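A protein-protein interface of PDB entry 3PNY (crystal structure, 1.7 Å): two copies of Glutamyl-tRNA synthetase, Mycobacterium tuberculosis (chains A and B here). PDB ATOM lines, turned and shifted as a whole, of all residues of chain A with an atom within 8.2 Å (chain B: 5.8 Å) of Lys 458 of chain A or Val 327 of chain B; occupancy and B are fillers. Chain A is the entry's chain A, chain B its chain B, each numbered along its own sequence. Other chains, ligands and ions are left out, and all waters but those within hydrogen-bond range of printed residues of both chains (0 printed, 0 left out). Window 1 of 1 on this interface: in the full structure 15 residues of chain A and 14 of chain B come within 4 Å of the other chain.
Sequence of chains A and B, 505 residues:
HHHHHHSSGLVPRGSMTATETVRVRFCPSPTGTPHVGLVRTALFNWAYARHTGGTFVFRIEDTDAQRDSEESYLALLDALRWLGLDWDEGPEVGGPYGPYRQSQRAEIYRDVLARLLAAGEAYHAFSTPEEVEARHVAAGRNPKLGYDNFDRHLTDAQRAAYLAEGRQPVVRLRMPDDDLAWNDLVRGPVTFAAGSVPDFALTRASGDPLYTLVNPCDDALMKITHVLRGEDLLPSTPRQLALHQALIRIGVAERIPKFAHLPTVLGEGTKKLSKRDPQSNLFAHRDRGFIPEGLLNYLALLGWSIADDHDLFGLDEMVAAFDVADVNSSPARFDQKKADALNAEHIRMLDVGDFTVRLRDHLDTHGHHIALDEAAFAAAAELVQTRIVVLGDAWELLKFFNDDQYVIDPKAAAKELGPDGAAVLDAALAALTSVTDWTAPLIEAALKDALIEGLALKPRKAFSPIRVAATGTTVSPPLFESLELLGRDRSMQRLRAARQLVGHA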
ATOM      1  N   LEU A 447      33.579 -24.725  -0.573  1.00  0.00           N
ATOM      2  CA  LEU A 447      32.115 -24.854  -0.705  1.00  0.00           C
ATOM      3  C   LEU A 447      31.706 -24.878  -2.175  1.00  0.00           C
ATOM      4  O   LEU A 447      30.814 -25.632  -2.574  1.00  0.00           O
ATOM      5  CB  LEU A 447      31.344 -23.727  -0.002  1.00  0.00           C
ATOM      6  CG  LEU A 447      31.077 -23.724   1.506  1.00  0.00           C
ATOM      7  CD1 LEU A 447      29.652 -24.110   1.887  1.00  0.00           C
ATOM      8  CD2 LEU A 447      32.091 -24.539   2.259  1.00  0.00           C
ATOM      9  N   LYS A 448      32.339 -24.026  -2.976  1.00  0.00           N
ATOM     10  CA  LYS A 448      32.005 -23.997  -4.399  1.00  0.00           C
ATOM     11  C   LYS A 448      32.425 -25.349  -4.991  1.00  0.00           C
ATOM     12  O   LYS A 448      31.702 -25.938  -5.723  1.00  0.00           O
ATOM     13  CB  LYS A 448      32.630 -22.808  -5.141  1.00  0.00           C
ATOM     14  CG  LYS A 448      31.821 -21.462  -5.047  1.00  0.00           C
ATOM     15  CD  LYS A 448      32.703 -20.177  -5.143  1.00  0.00           C
ATOM     16  CE  LYS A 448      32.157 -19.100  -6.067  1.00  0.00           C
ATOM     17  NZ  LYS A 448      31.277 -18.154  -5.390  1.00  0.00           N
ATOM     18  N   LEU A 451      29.447 -27.748  -3.809  1.00  0.00           N
ATOM     19  CA  LEU A 451      28.037 -27.382  -3.912  1.00  0.00           C
ATOM     20  C   LEU A 451      27.591 -26.838  -5.280  1.00  0.00           C
ATOM     21  O   LEU A 451      26.536 -27.147  -5.733  1.00  0.00           O
ATOM     22  CB  LEU A 451      27.629 -26.426  -2.795  1.00  0.00           C
ATOM     23  CG  LEU A 451      27.645 -27.156  -1.434  1.00  0.00           C
ATOM     24  CD1 LEU A 451      28.143 -26.279  -0.303  1.00  0.00           C
ATOM     25  CD2 LEU A 451      26.314 -27.748  -1.136  1.00  0.00           C
ATOM     26  N   ILE A 452      28.440 -26.026  -5.900  1.00  0.00           N
ATOM     27  CA  ILE A 452      28.425 -25.865  -7.349  1.00  0.00           C
ATOM     28  C   ILE A 452      29.044 -27.072  -8.045  1.00  0.00           C
ATOM     29  O   ILE A 452      28.513 -27.566  -9.040  1.00  0.00           O
ATOM     30  CB  ILE A 452      29.178 -24.593  -7.783  1.00  0.00           C
ATOM     31  CG1 ILE A 452      28.641 -23.373  -7.034  1.00  0.00           C
ATOM     32  CG2 ILE A 452      29.065 -24.394  -9.287  1.00  0.00           C
ATOM     33  CD1 ILE A 452      29.198 -22.056  -7.530  1.00  0.00           C
ATOM     34  N   GLU A 453      30.168 -27.543  -7.515  1.00  0.00           N
ATOM     35  CA  GLU A 453      31.046 -28.442  -8.254  1.00  0.00           C
ATOM     36  C   GLU A 453      30.358 -29.774  -8.538  1.00  0.00           C
ATOM     37  O   GLU A 453      30.396 -30.275  -9.661  1.00  0.00           O
ATOM     38  CB  GLU A 453      32.346 -28.675  -7.483  1.00  0.00           C
ATOM     39  CG  GLU A 453      33.286 -27.481  -7.475  1.00  0.00           C
ATOM     40  CD  GLU A 453      33.887 -27.204  -8.839  1.00  0.00           C
ATOM     41  OE1 GLU A 453      34.338 -28.165  -9.498  1.00  0.00           O
ATOM     42  OE2 GLU A 453      33.909 -26.026  -9.253  1.00  0.00           O
ATOM     43  N   LEU A 455      27.213 -30.861  -6.714  1.00  0.00           N
ATOM     44  CA  LEU A 455      25.761 -30.824  -6.587  1.00  0.00           C
ATOM     45  C   LEU A 455      25.178 -30.164  -7.857  1.00  0.00           C
ATOM     46  O   LEU A 455      23.973 -30.282  -8.042  1.00  0.00           O
ATOM     47  CB  LEU A 455      25.357 -30.232  -5.235  1.00  0.00           C
ATOM     48  CG  LEU A 455      25.840 -30.985  -3.994  1.00  0.00           C
ATOM     49  CD1 LEU A 455      25.518 -30.203  -2.730  1.00  0.00           C
ATOM     50  CD2 LEU A 455      25.230 -32.377  -3.937  1.00  0.00           C
ATOM     51  N   ALA A 456      26.056 -29.310  -8.377  1.00  0.00           N
ATOM     52  CA  ALA A 456      25.857 -28.626  -9.649  1.00  0.00           C
ATOM     53  C   ALA A 456      24.705 -27.605  -9.627  1.00  0.00           C
ATOM     54  O   ALA A 456      24.342 -27.157 -10.692  1.00  0.00           O
ATOM     55  CB  ALA A 456      25.577 -29.633 -10.755  1.00  0.00           C
ATOM     56  N   LEU A 457      24.258 -26.972  -8.551  1.00  0.00           N
ATOM     57  CA  LEU A 457      23.341 -25.839  -8.505  1.00  0.00           C
ATOM     58  C   LEU A 457      24.097 -24.525  -8.338  1.00  0.00           C
ATOM     59  O   LEU A 457      25.307 -24.517  -8.116  1.00  0.00           O
ATOM     60  CB  LEU A 457      22.330 -26.013  -7.369  1.00  0.00           C
ATOM     61  CG  LEU A 457      20.872 -26.218  -7.785  1.00  0.00           C
ATOM     62  CD1 LEU A 457      19.930 -25.781  -6.674  1.00  0.00           C
ATOM     63  CD2 LEU A 457      20.570 -25.470  -9.074  1.00  0.00           C
ATOM     64  N   LYS A 458      23.373 -23.415  -8.446  1.00  0.00           N
ATOM     65  CA  LYS A 458      23.996 -22.111  -8.639  1.00  0.00           C
ATOM     66  C   LYS A 458      24.911 -21.759  -7.470  1.00  0.00           C
ATOM     67  O   LYS A 458      24.667 -22.167  -6.334  1.00  0.00           O
ATOM     68  CB  LYS A 458      22.929 -21.028  -8.816  1.00  0.00           C
ATOM     69  CG  LYS A 458      23.096 -20.194 -10.076  1.00  0.00           C
ATOM     70  CD  LYS A 458      21.800 -19.490 -10.447  1.00  0.00           C
ATOM     71  CE  LYS A 458      22.013 -18.509 -11.588  1.00  0.00           C
ATOM     72  NZ  LYS A 458      20.727 -17.945 -12.082  1.00  0.00           N
ATOM     73  N   PRO A 459      25.963 -20.999  -7.756  1.00  0.00           N
ATOM     74  CA  PRO A 459      26.904 -20.564  -6.719  1.00  0.00           C
ATOM     75  C   PRO A 459      26.189 -19.985  -5.505  1.00  0.00           C
ATOM     76  O   PRO A 459      26.730 -19.863  -4.438  1.00  0.00           O
ATOM     77  CB  PRO A 459      27.720 -19.477  -7.422  1.00  0.00           C
ATOM     78  CG  PRO A 459      26.808 -18.932  -8.464  1.00  0.00           C
ATOM     79  CD  PRO A 459      26.001 -20.102  -8.935  1.00  0.00           C
ATOM     80  N   ARG A 460      24.954 -19.550  -5.695  1.00  0.00           N
ATOM     81  CA  ARG A 460      24.165 -18.939  -4.631  1.00  0.00           C
ATOM     82  C   ARG A 460      23.396 -19.930  -3.768  1.00  0.00           C
ATOM     83  O   ARG A 460      22.693 -19.538  -2.833  1.00  0.00           O
ATOM     84  CB  ARG A 460      23.136 -17.973  -5.218  1.00  0.00           C
ATOM     85  CG  ARG A 460      22.362 -17.182  -4.173  1.00  0.00           C
ATOM     86  CD  ARG A 460      21.260 -16.307  -4.749  1.00  0.00           C
ATOM     87  NE  ARG A 460      19.960 -16.971  -4.716  1.00  0.00           N
ATOM     88  CZ  ARG A 460      19.002 -16.780  -5.611  1.00  0.00           C
ATOM     89  NH1 ARG A 460      19.216 -15.988  -6.654  1.00  0.00           N
ATOM     90  NH2 ARG A 460      17.829 -17.380  -5.470  1.00  0.00           N
ATOM     91  N   LYS A 461      23.532 -21.213  -4.083  1.00  0.00           N
ATOM     92  CA  LYS A 461      23.016 -22.272  -3.224  1.00  0.00           C
ATOM     93  C   LYS A 461      24.147 -23.126  -2.659  1.00  0.00           C
ATOM     94  O   LYS A 461      23.993 -23.771  -1.622  1.00  0.00           O
ATOM     95  CB  LYS A 461      22.027 -23.152  -3.992  1.00  0.00           C
ATOM     96  CG  LYS A 461      20.714 -22.462  -4.326  1.00  0.00           C
ATOM     97  CD  LYS A 461      19.766 -23.403  -5.051  1.00  0.00           C
ATOM     98  CE  LYS A 461      18.483 -22.693  -5.453  1.00  0.00           C
ATOM     99  NZ  LYS A 461      17.548 -23.601  -6.173  1.00  0.00           N
ATOM    100  N   ALA A 462      25.283 -23.125  -3.348  1.00  0.00           N
ATOM    101  CA  ALA A 462      26.560 -23.445  -2.722  1.00  0.00           C
ATOM    102  C   ALA A 462      26.706 -22.741  -1.377  1.00  0.00           C
ATOM    103  O   ALA A 462      27.000 -23.374  -0.363  1.00  0.00           O
ATOM    104  CB  ALA A 462      27.711 -23.074  -3.644  1.00  0.00           C
ATOM    105  N   PHE A 463      26.498 -21.428  -1.376  1.00  0.00           N
ATOM    106  CA  PHE A 463      26.805 -20.610  -0.222  1.00  0.00           C
ATOM    107  C   PHE A 463      25.646 -20.272   0.665  1.00  0.00           C
ATOM    108  O   PHE A 463      25.802 -20.074   1.851  1.00  0.00           O
ATOM    109  CB  PHE A 463      27.601 -19.416  -0.656  1.00  0.00           C
ATOM    110  CG  PHE A 463      28.904 -19.811  -1.214  1.00  0.00           C
ATOM    111  CD1 PHE A 463      29.794 -20.504  -0.425  1.00  0.00           C
ATOM    112  CD2 PHE A 463      29.212 -19.592  -2.516  1.00  0.00           C
ATOM    113  CE1 PHE A 463      30.939 -20.899  -0.914  1.00  0.00           C
ATOM    114  CE2 PHE A 463      30.387 -19.985  -3.007  1.00  0.00           C
ATOM    115  CZ  PHE A 463      31.252 -20.640  -2.218  1.00  0.00           C
ATOM    116  N   SER A 464      24.469 -20.243   0.082  1.00  0.00           N
ATOM    117  CA  SER A 464      23.296 -19.922   0.824  1.00  0.00           C
ATOM    118  C   SER A 464      23.168 -20.651   2.150  1.00  0.00           C
ATOM    119  O   SER A 464      23.180 -20.032   3.191  1.00  0.00           O
ATOM    120  CB  SER A 464      22.056 -20.123   0.006  1.00  0.00           C
ATOM    121  OG  SER A 464      20.974 -19.487   0.637  1.00  0.00           O
ATOM    122  N   PRO A 465      22.969 -21.957   2.110  1.00  0.00           N
ATOM    123  CA  PRO A 465      22.513 -22.630   3.324  1.00  0.00           C
ATOM    124  C   PRO A 465      23.588 -22.549   4.353  1.00  0.00           C
ATOM    125  O   PRO A 465      23.303 -22.700   5.527  1.00  0.00           O
ATOM    126  CB  PRO A 465      22.273 -24.089   2.880  1.00  0.00           C
ATOM    127  CG  PRO A 465      22.781 -24.191   1.484  1.00  0.00           C
ATOM    128  CD  PRO A 465      22.850 -22.808   0.917  1.00  0.00           C
ATOM    129  N   PHE B  44      29.315 -10.270 -21.969  1.00  0.00           N
ATOM    130  CA  PHE B  44      29.148 -11.295 -20.945  1.00  0.00           C
ATOM    131  C   PHE B  44      30.008 -12.518 -21.246  1.00  0.00           C
ATOM    132  O   PHE B  44      30.514 -13.173 -20.334  1.00  0.00           O
ATOM    133  CB  PHE B  44      27.678 -11.701 -20.828  1.00  0.00           C
ATOM    134  CG  PHE B  44      26.909 -10.907 -19.812  1.00  0.00           C
ATOM    135  CD1 PHE B  44      27.306  -9.624 -19.470  1.00  0.00           C
ATOM    136  CD2 PHE B  44      25.788 -11.441 -19.198  1.00  0.00           C
ATOM    137  CE1 PHE B  44      26.600  -8.891 -18.536  1.00  0.00           C
ATOM    138  CE2 PHE B  44      25.079 -10.713 -18.263  1.00  0.00           C
ATOM    139  CZ  PHE B  44      25.485  -9.435 -17.932  1.00  0.00           C
ATOM    140  N   LEU B 185      23.128 -22.573 -16.507  1.00  0.00           N
ATOM    141  CA  LEU B 185      23.946 -21.887 -15.514  1.00  0.00           C
ATOM    142  C   LEU B 185      23.233 -20.653 -14.971  1.00  0.00           C
ATOM    143  O   LEU B 185      23.589 -20.135 -13.913  1.00  0.00           O
ATOM    144  CB  LEU B 185      25.297 -21.493 -16.112  1.00  0.00           C
ATOM    145  CG  LEU B 185      26.206 -22.644 -16.551  1.00  0.00           C
ATOM    146  CD1 LEU B 185      27.356 -22.126 -17.401  1.00  0.00           C
ATOM    147  CD2 LEU B 185      26.728 -23.407 -15.343  1.00  0.00           C
ATOM    148  N   VAL B 186      22.226 -20.188 -15.702  1.00  0.00           N
ATOM    149  CA  VAL B 186      21.400 -19.075 -15.247  1.00  0.00           C
ATOM    150  C   VAL B 186      20.032 -19.559 -14.778  1.00  0.00           C
ATOM    151  O   VAL B 186      19.546 -19.150 -13.724  1.00  0.00           O
ATOM    152  CB  VAL B 186      21.210 -18.024 -16.357  1.00  0.00           C
ATOM    153  CG1 VAL B 186      20.211 -16.965 -15.918  1.00  0.00           C
ATOM    154  CG2 VAL B 186      22.544 -17.390 -16.721  1.00  0.00           C
ATOM    155  N   ARG B 187      19.416 -20.432 -15.568  1.00  0.00           N
ATOM    156  CA  ARG B 187      17.994 -20.725 -15.425  1.00  0.00           C
ATOM    157  C   ARG B 187      17.767 -21.906 -14.486  1.00  0.00           C
ATOM    158  O   ARG B 187      16.637 -22.186 -14.088  1.00  0.00           O
ATOM    159  CB  ARG B 187      17.366 -21.011 -16.789  1.00  0.00           C
ATOM    160  CG  ARG B 187      17.255 -19.790 -17.689  1.00  0.00           C
ATOM    161  CD  ARG B 187      16.043 -18.946 -17.328  1.00  0.00           C
ATOM    162  NE  ARG B 187      14.790 -19.619 -17.660  1.00  0.00           N
ATOM    163  CZ  ARG B 187      14.054 -19.341 -18.731  1.00  0.00           C
ATOM    164  NH1 ARG B 187      14.444 -18.399 -19.581  1.00  0.00           N
ATOM    165  NH2 ARG B 187      12.928 -20.004 -18.955  1.00  0.00           N
ATOM    166  N   GLY B 188      18.850 -22.594 -14.137  1.00  0.00           N
ATOM    167  CA  GLY B 188      18.753 -23.879 -13.469  1.00  0.00           C
ATOM    168  C   GLY B 188      18.309 -24.987 -14.404  1.00  0.00           C
ATOM    169  O   GLY B 188      18.287 -24.813 -15.622  1.00  0.00           O
ATOM    170  N   HIS B 261      21.503 -19.028 -20.304  1.00  0.00           N
ATOM    171  CA  HIS B 261      20.597 -18.243 -21.134  1.00  0.00           C
ATOM    172  C   HIS B 261      20.256 -16.912 -20.473  1.00  0.00           C
ATOM    173  O   HIS B 261      19.618 -16.876 -19.420  1.00  0.00           O
ATOM    174  CB  HIS B 261      19.317 -19.030 -21.422  1.00  0.00           C
ATOM    175  CG  HIS B 261      19.450 -20.012 -22.544  1.00  0.00           C
ATOM    176  ND1 HIS B 261      19.819 -21.324 -22.346  1.00  0.00           N
ATOM    177  CD2 HIS B 261      19.264 -19.871 -23.878  1.00  0.00           C
ATOM    178  CE1 HIS B 261      19.854 -21.950 -23.509  1.00  0.00           C
ATOM    179  NE2 HIS B 261      19.521 -21.091 -24.454  1.00  0.00           N
ATOM    180  N   LEU B 262      20.685 -15.820 -21.096  1.00  0.00           N
ATOM    181  CA  LEU B 262      20.695 -14.518 -20.442  1.00  0.00           C
ATOM    182  C   LEU B 262      19.330 -13.845 -20.531  1.00  0.00           C
ATOM    183  O   LEU B 262      18.666 -13.902 -21.566  1.00  0.00           O
ATOM    184  CB  LEU B 262      21.767 -13.616 -21.058  1.00  0.00           C
ATOM    185  CG  LEU B 262      23.166 -14.220 -21.193  1.00  0.00           C
ATOM    186  CD1 LEU B 262      24.068 -13.311 -22.014  1.00  0.00           C
ATOM    187  CD2 LEU B 262      23.771 -14.489 -19.823  1.00  0.00           C
ATOM    188  N   PRO B 263      18.916 -13.208 -19.440  1.00  0.00           N
ATOM    189  CA  PRO B 263      17.633 -12.500 -19.400  1.00  0.00           C
ATOM    190  C   PRO B 263      17.497 -11.507 -20.549  1.00  0.00           C
ATOM    191  O   PRO B 263      18.212 -10.505 -20.585  1.00  0.00           O
ATOM    192  CB  PRO B 263      17.691 -11.755 -18.065  1.00  0.00           C
ATOM    193  CG  PRO B 263      19.143 -11.538 -17.825  1.00  0.00           C
ATOM    194  CD  PRO B 263      19.837 -12.747 -18.385  1.00  0.00           C
ATOM    195  N   LEU B 302      22.780  -5.439 -16.615  1.00  0.00           N
ATOM    196  CA  LEU B 302      21.592  -6.057 -17.191  1.00  0.00           C
ATOM    197  C   LEU B 302      21.585  -7.564 -16.954  1.00  0.00           C
ATOM    198  O   LEU B 302      21.733  -8.350 -17.890  1.00  0.00           O
ATOM    199  CB  LEU B 302      21.505  -5.760 -18.689  1.00  0.00           C
ATOM    200  CG  LEU B 302      21.334  -4.290 -19.079  1.00  0.00           C
ATOM    201  CD1 LEU B 302      21.436  -4.120 -20.587  1.00  0.00           C
ATOM    202  CD2 LEU B 302      20.011  -3.748 -18.562  1.00  0.00           C
ATOM    203  N   GLY B 303      21.409  -7.960 -15.697  1.00  0.00           N
ATOM    204  CA  GLY B 303      21.252  -9.387 -15.346  1.00  0.00           C
ATOM    205  C   GLY B 303      22.285  -9.780 -14.311  1.00  0.00           C
ATOM    206  O   GLY B 303      22.379 -10.943 -13.974  1.00  0.00           O
ATOM    207  N   TRP B 304      23.047  -8.809 -13.819  1.00  0.00           N
ATOM    208  CA  TRP B 304      24.237  -9.096 -13.027  1.00  0.00           C
ATOM    209  C   TRP B 304      24.576  -7.934 -12.101  1.00  0.00           C
ATOM    210  O   TRP B 304      24.312  -6.774 -12.420  1.00  0.00           O
ATOM    211  CB  TRP B 304      25.426  -9.405 -13.940  1.00  0.00           C
ATOM    212  CG  TRP B 304      26.639  -9.887 -13.203  1.00  0.00           C
ATOM    213  CD1 TRP B 304      26.813 -11.110 -12.625  1.00  0.00           C
ATOM    214  CD2 TRP B 304      27.845  -9.153 -12.964  1.00  0.00           C
ATOM    215  NE1 TRP B 304      28.056 -11.184 -12.041  1.00  0.00           N
ATOM    216  CE2 TRP B 304      28.709  -9.995 -12.235  1.00  0.00           C
ATOM    217  CE3 TRP B 304      28.281  -7.866 -13.296  1.00  0.00           C
ATOM    218  CZ2 TRP B 304      29.981  -9.593 -11.832  1.00  0.00           C
ATOM    219  CZ3 TRP B 304      29.543  -7.469 -12.895  1.00  0.00           C
ATOM    220  CH2 TRP B 304      30.378  -8.329 -12.171  1.00  0.00           C
ATOM    221  N   PHE B 322      33.481 -11.742 -12.566  1.00  0.00           N
ATOM    222  CA  PHE B 322      32.325 -12.203 -13.325  1.00  0.00           C
ATOM    223  C   PHE B 322      32.313 -13.723 -13.445  1.00  0.00           C
ATOM    224  O   PHE B 322      33.253 -14.322 -13.969  1.00  0.00           O
ATOM    225  CB  PHE B 322      32.310 -11.566 -14.717  1.00  0.00           C
ATOM    226  CG  PHE B 322      31.061 -11.852 -15.500  1.00  0.00           C
ATOM    227  CD1 PHE B 322      31.045 -12.846 -16.465  1.00  0.00           C
ATOM    228  CD2 PHE B 322      29.904 -11.126 -15.274  1.00  0.00           C
ATOM    229  CE1 PHE B 322      29.898 -13.112 -17.187  1.00  0.00           C
ATOM    230  CE2 PHE B 322      28.753 -11.387 -15.994  1.00  0.00           C
ATOM    231  CZ  PHE B 322      28.750 -12.381 -16.952  1.00  0.00           C
ATOM    232  N   ASP B 323      31.244 -14.342 -12.955  1.00  0.00           N
ATOM    233  CA  ASP B 323      30.930 -15.722 -13.306  1.00  0.00           C
ATOM    234  C   ASP B 323      29.460 -15.875 -13.680  1.00  0.00           C
ATOM    235  O   ASP B 323      28.572 -15.568 -12.885  1.00  0.00           O
ATOM    236  CB  ASP B 323      31.279 -16.662 -12.151  1.00  0.00           C
ATOM    237  CG  ASP B 323      30.525 -17.975 -12.219  1.00  0.00           C
ATOM    238  OD1 ASP B 323      30.091 -18.356 -13.327  1.00  0.00           O
ATOM    239  OD2 ASP B 323      30.366 -18.626 -11.166  1.00  0.00           O
ATOM    240  N   VAL B 324      29.210 -16.351 -14.895  1.00  0.00           N
ATOM    241  CA  VAL B 324      27.890 -16.240 -15.505  1.00  0.00           C
ATOM    242  C   VAL B 324      26.830 -16.938 -14.658  1.00  0.00           C
ATOM    243  O   VAL B 324      25.640 -16.646 -14.772  1.00  0.00           O
ATOM    244  CB  VAL B 324      27.873 -16.836 -16.925  1.00  0.00           C
ATOM    245  CG1 VAL B 324      28.047 -18.346 -16.869  1.00  0.00           C
ATOM    246  CG2 VAL B 324      26.581 -16.469 -17.638  1.00  0.00           C
ATOM    247  N   ALA B 325      27.272 -17.861 -13.810  1.00  0.00           N
ATOM    248  CA  ALA B 325      26.368 -18.569 -12.911  1.00  0.00           C
ATOM    249  C   ALA B 325      25.793 -17.631 -11.856  1.00  0.00           C
ATOM    250  O   ALA B 325      24.861 -17.989 -11.135  1.00  0.00           O
ATOM    251  CB  ALA B 325      27.086 -19.737 -12.251  1.00  0.00           C
ATOM    252  N   ASP B 326      26.354 -16.429 -11.770  1.00  0.00           N
ATOM    253  CA  ASP B 326      25.835 -15.398 -10.863  1.00  0.00           C
ATOM    254  C   ASP B 326      24.816 -14.512 -11.560  1.00  0.00           C
ATOM    255  O   ASP B 326      24.098 -13.704 -10.957  1.00  0.00           O
ATOM    256  CB  ASP B 326      26.978 -14.581 -10.313  1.00  0.00           C
ATOM    257  CG  ASP B 326      27.729 -15.275  -9.228  1.00  0.00           C
ATOM    258  OD1 ASP B 326      27.104 -16.065  -8.429  1.00  0.00           O
ATOM    259  OD2 ASP B 326      28.935 -15.069  -9.133  1.00  0.00           O
ATOM    260  N   VAL B 327      24.773 -14.578 -12.889  1.00  0.00           N
ATOM    261  CA  VAL B 327      23.677 -13.889 -13.564  1.00  0.00           C
ATOM    262  C   VAL B 327      22.300 -14.278 -13.146  1.00  0.00           C
ATOM    263  O   VAL B 327      22.007 -15.442 -12.889  1.00  0.00           O
ATOM    264  CB  VAL B 327      23.866 -14.067 -15.098  1.00  0.00           C
ATOM    265  CG1 VAL B 327      22.644 -13.563 -15.834  1.00  0.00           C
ATOM    266  CG2 VAL B 327      25.232 -13.412 -15.405  1.00  0.00           C
ATOM    267  N   ASN B 328      21.413 -13.320 -13.022  1.00  0.00           N
ATOM    268  CA  ASN B 328      20.112 -13.730 -12.516  1.00  0.00           C
ATOM    269  C   ASN B 328      19.080 -13.852 -13.642  1.00  0.00           C
ATOM    270  O   ASN B 328      19.345 -13.340 -14.738  1.00  0.00           O
ATOM    271  CB  ASN B 328      19.726 -12.844 -11.356  1.00  0.00           C
ATOM    272  CG  ASN B 328      19.588 -11.419 -11.769  1.00  0.00           C
ATOM    273  OD1 ASN B 328      20.350 -10.536 -11.337  1.00  0.00           O
ATOM    274  ND2 ASN B 328      18.584 -11.161 -12.581  1.00  0.00           N
ATOM    275  N   SER B 329      18.006 -14.613 -13.430  1.00  0.00           N
ATOM    276  CA  SER B 329      17.047 -14.886 -14.499  1.00  0.00           C
ATOM    277  C   SER B 329      15.852 -13.948 -14.507  1.00  0.00           C
ATOM    278  O   SER B 329      14.985 -14.054 -15.349  1.00  0.00           O
ATOM    279  CB  SER B 329      16.597 -16.359 -14.506  1.00  0.00           C
ATOM    280  OG  SER B 329      16.802 -16.973 -13.215  1.00  0.00           O
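O of Val 327 of chain B is in hydrogen-bond range of NZ of Lys 458 of chain A (2.9 Å). The side-chain amino group (NZ) of Lys 458 of chain A lies close to the backbone carbonyl oxygen (O) of Val 186 of chain B.
The backbone NH of Ala 325 of chain B sits at hydrogen-bond distance from the side-chain carboxylate of Asp 323 of chain B (2.9 Å).
Lys 458 of chain A touches Leu 185 of chain B (CE to O, 3.2 Å). Lys 458 of chain A touches Ala 325 of chain B. Pro 459 of chain A touches Ala 325 of chain B (CD to O, 3.3 Å). Pro 459 of chain A touches Asp 326 of chain B (CG to OD1, 2.9 Å).
Of chain B, only Leu 185 (3.2 Å), Val 186 (2.4 Å), Ala 325 (2.9 Å) and Val 327 (2.9 Å) come within 4 Å of Lys 458 of chain A. Of chain A, only Lys 458 (2.9 Å) comes within 4 Å of Val 327 of chain B. Of the printed residues of chain A, Leu 185 of chain B touches Lys 458. Of the printed residues of chain A, Val 186 of chain B touches Lys 458. Ser 329 of chain B touches none of the printed residues of chain A. The nearest residue of chain B that does not touch Lys 458 of chain A is Ser 329 of chain B (4.2 Å). The nearest residue of chain A that does not touch Val 327 of chain B is Pro 459 of chain A (6.5 Å).
Printed residues of chain B that touch a printed residue of chain A: Leu 185, Val 186, Ala 325, Asp 326 and Val 327. Hydrophobic or aromatic side chains of chain B within 4 Å of the printed part of chain A: Val 186 and Ala 325. Among the printed residues, no Asp or Glu carboxylate lies within 4 Å of a Lys or Arg side-chain nitrogen of the other chain.
No position is printed for both chains.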
